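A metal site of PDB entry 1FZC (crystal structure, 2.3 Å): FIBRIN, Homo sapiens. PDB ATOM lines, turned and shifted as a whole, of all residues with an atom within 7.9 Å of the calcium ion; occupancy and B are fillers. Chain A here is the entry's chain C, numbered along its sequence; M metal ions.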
ATOM      1  N   SER A 226       5.534 -17.641  -0.986  1.00  0.00           N
ATOM      2  CA  SER A 226       6.915 -18.030  -1.248  1.00  0.00           C
ATOM      3  C   SER A 226       6.998 -19.232  -2.230  1.00  0.00           C
ATOM      4  O   SER A 226       6.156 -20.087  -2.320  1.00  0.00           O
ATOM      5  CB  SER A 226       7.646 -18.488   0.047  1.00  0.00           C
ATOM      6  OG  SER A 226       7.989 -17.510   0.998  1.00  0.00           O
ATOM      7  N   ASN A 230      11.905 -17.214  -4.642  1.00  0.00           N
ATOM      8  CA  ASN A 230      11.335 -16.035  -4.045  1.00  0.00           C
ATOM      9  C   ASN A 230      10.819 -16.382  -2.641  1.00  0.00           C
ATOM     10  O   ASN A 230       9.629 -16.615  -2.347  1.00  0.00           O
ATOM     11  CB  ASN A 230      10.167 -15.478  -4.880  1.00  0.00           C
ATOM     12  CG  ASN A 230      10.040 -13.966  -4.918  1.00  0.00           C
ATOM     13  OD1 ASN A 230      10.292 -13.354  -5.971  1.00  0.00           O
ATOM     14  ND2 ASN A 230       9.678 -13.274  -3.895  1.00  0.00           N
ATOM     15  N   ASP A 231      11.779 -16.331  -1.708  1.00  0.00           N
ATOM     16  CA  ASP A 231      11.562 -16.638  -0.306  1.00  0.00           C
ATOM     17  C   ASP A 231      11.064 -15.418   0.468  1.00  0.00           C
ATOM     18  O   ASP A 231      11.733 -14.368   0.513  1.00  0.00           O
ATOM     19  CB  ASP A 231      12.902 -17.135   0.237  1.00  0.00           C
ATOM     20  CG  ASP A 231      12.980 -17.358   1.747  1.00  0.00           C
ATOM     21  OD1 ASP A 231      11.992 -17.125   2.497  1.00  0.00           O
ATOM     22  OD2 ASP A 231      14.058 -17.830   2.184  1.00  0.00           O
ATOM     23  N   ASN A 232       9.909 -15.517   1.102  1.00  0.00           N
ATOM     24  CA  ASN A 232       9.380 -14.414   1.933  1.00  0.00           C
ATOM     25  C   ASN A 232       8.809 -15.037   3.227  1.00  0.00           C
ATOM     26  O   ASN A 232       7.751 -14.671   3.744  1.00  0.00           O
ATOM     27  CB  ASN A 232       8.283 -13.696   1.179  1.00  0.00           C
ATOM     28  CG  ASN A 232       8.601 -13.336  -0.238  1.00  0.00           C
ATOM     29  OD1 ASN A 232       8.207 -14.008  -1.212  1.00  0.00           O
ATOM     30  ND2 ASN A 232       9.321 -12.253  -0.486  1.00  0.00           N
ATOM     31  N   ASP A 233       9.459 -16.149   3.650  1.00  0.00           N
ATOM     32  CA  ASP A 233       8.929 -16.887   4.835  1.00  0.00           C
ATOM     33  C   ASP A 233       9.518 -16.286   6.096  1.00  0.00           C
ATOM     34  O   ASP A 233      10.377 -15.395   6.015  1.00  0.00           O
ATOM     35  CB  ASP A 233       9.122 -18.398   4.649  1.00  0.00           C
ATOM     36  CG  ASP A 233      10.587 -18.816   4.613  1.00  0.00           C
ATOM     37  OD1 ASP A 233      11.521 -18.137   5.058  1.00  0.00           O
ATOM     38  OD2 ASP A 233      11.002 -19.887   4.088  1.00  0.00           O
ATOM     39  N   LYS A 234       9.141 -16.702   7.300  1.00  0.00           N
ATOM     40  CA  LYS A 234       9.715 -16.182   8.529  1.00  0.00           C
ATOM     41  C   LYS A 234      10.880 -17.073   8.999  1.00  0.00           C
ATOM     42  O   LYS A 234      11.153 -17.116  10.203  1.00  0.00           O
ATOM     43  CB  LYS A 234       8.699 -16.102   9.659  1.00  0.00           C
ATOM     44  CG  LYS A 234       7.353 -15.520   9.334  1.00  0.00           C
ATOM     45  CD  LYS A 234       7.573 -14.077   8.889  1.00  0.00           C
ATOM     46  CE  LYS A 234       6.431 -13.223   9.418  1.00  0.00           C
ATOM     47  NZ  LYS A 234       6.451 -11.924   8.672  1.00  0.00           N
ATOM     48  N   PHE A 235      11.466 -17.862   8.094  1.00  0.00           N
ATOM     49  CA  PHE A 235      12.494 -18.813   8.461  1.00  0.00           C
ATOM     50  C   PHE A 235      13.850 -18.336   8.009  1.00  0.00           C
ATOM     51  O   PHE A 235      14.055 -17.618   7.024  1.00  0.00           O
ATOM     52  CB  PHE A 235      12.200 -20.215   7.923  1.00  0.00           C
ATOM     53  CG  PHE A 235      13.196 -21.321   8.085  1.00  0.00           C
ATOM     54  CD1 PHE A 235      13.952 -21.436   9.240  1.00  0.00           C
ATOM     55  CD2 PHE A 235      13.391 -22.290   7.102  1.00  0.00           C
ATOM     56  CE1 PHE A 235      14.856 -22.469   9.404  1.00  0.00           C
ATOM     57  CE2 PHE A 235      14.299 -23.333   7.275  1.00  0.00           C
ATOM     58  CZ  PHE A 235      15.028 -23.424   8.438  1.00  0.00           C
ATOM     59  N   GLU A 236      14.884 -18.780   8.683  1.00  0.00           N
ATOM     60  CA  GLU A 236      16.265 -18.420   8.331  1.00  0.00           C
ATOM     61  C   GLU A 236      16.698 -19.094   7.035  1.00  0.00           C
ATOM     62  O   GLU A 236      17.425 -18.528   6.223  1.00  0.00           O
ATOM     63  CB  GLU A 236      17.152 -18.758   9.530  1.00  0.00           C
ATOM     64  CG  GLU A 236      16.649 -19.994  10.290  1.00  0.00           C
ATOM     65  CD  GLU A 236      15.775 -19.735  11.513  1.00  0.00           C
ATOM     66  OE1 GLU A 236      14.989 -18.774  11.555  1.00  0.00           O
ATOM     67  OE2 GLU A 236      15.862 -20.556  12.452  1.00  0.00           O
ATOM     68  N   GLY A 237      16.236 -20.321   6.791  1.00  0.00           N
ATOM     69  CA  GLY A 237      16.413 -21.000   5.534  1.00  0.00           C
ATOM     70  C   GLY A 237      15.203 -20.660   4.619  1.00  0.00           C
ATOM     71  O   GLY A 237      14.510 -19.607   4.729  1.00  0.00           O
ATOM     72  N   ASN A 238      14.982 -21.556   3.666  1.00  0.00           N
ATOM     73  CA  ASN A 238      13.958 -21.472   2.638  1.00  0.00           C
ATOM     74  C   ASN A 238      12.961 -22.610   2.749  1.00  0.00           C
ATOM     75  O   ASN A 238      13.248 -23.643   2.165  1.00  0.00           O
ATOM     76  CB  ASN A 238      14.575 -21.593   1.235  1.00  0.00           C
ATOM     77  CG  ASN A 238      13.769 -21.174   0.006  1.00  0.00           C
ATOM     78  OD1 ASN A 238      14.423 -20.461  -0.794  1.00  0.00           O
ATOM     79  ND2 ASN A 238      12.522 -21.576  -0.198  1.00  0.00           N
ATOM     80  N   CYS A 239      11.810 -22.348   3.354  1.00  0.00           N
ATOM     81  CA  CYS A 239      10.746 -23.337   3.454  1.00  0.00           C
ATOM     82  C   CYS A 239      10.295 -23.849   2.077  1.00  0.00           C
ATOM     83  O   CYS A 239      10.191 -25.050   1.787  1.00  0.00           O
ATOM     84  CB  CYS A 239       9.548 -22.698   4.175  1.00  0.00           C
ATOM     85  SG  CYS A 239       9.705 -22.199   5.906  1.00  0.00           S
ATOM     86  N   ALA A 240      10.025 -22.902   1.153  1.00  0.00           N
ATOM     87  CA  ALA A 240       9.533 -23.325  -0.169  1.00  0.00           C
ATOM     88  C   ALA A 240      10.557 -24.239  -0.855  1.00  0.00           C
ATOM     89  O   ALA A 240      10.080 -25.231  -1.407  1.00  0.00           O
ATOM     90  CB  ALA A 240       9.107 -22.189  -1.096  1.00  0.00           C
ATOM     91  N   ASN A 250       5.442 -19.855   6.835  1.00  0.00           N
ATOM     92  CA  ASN A 250       5.764 -19.101   8.077  1.00  0.00           C
ATOM     93  C   ASN A 250       7.101 -19.676   8.541  1.00  0.00           C
ATOM     94  O   ASN A 250       8.177 -19.324   8.017  1.00  0.00           O
ATOM     95  CB  ASN A 250       4.580 -19.252   9.004  1.00  0.00           C
ATOM     96  CG  ASN A 250       4.713 -18.538  10.338  1.00  0.00           C
ATOM     97  OD1 ASN A 250       5.801 -18.080  10.750  1.00  0.00           O
ATOM     98  ND2 ASN A 250       3.591 -18.459  11.055  1.00  0.00           N
HETATM   99 CA    CA M   1      13.639 -17.440   4.464  1.00  0.00          CA
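OG of Ser 226 is in hydrogen-bond range of N of Asp 233.
The backbone NH (N) of Cys 239 lies within hydrogen-bond range of the side-chain carboxylate (OD2) of Asp 233 (2.7 Å).
Of the 13 residues printed, 4 come within 4 Å of the calcium ion.
The calcium ion is bound by OD1 of Asp 233, OD2 of Asp 231, O of Gly 237, OD1 of Asp 231 and O of Phe 235.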
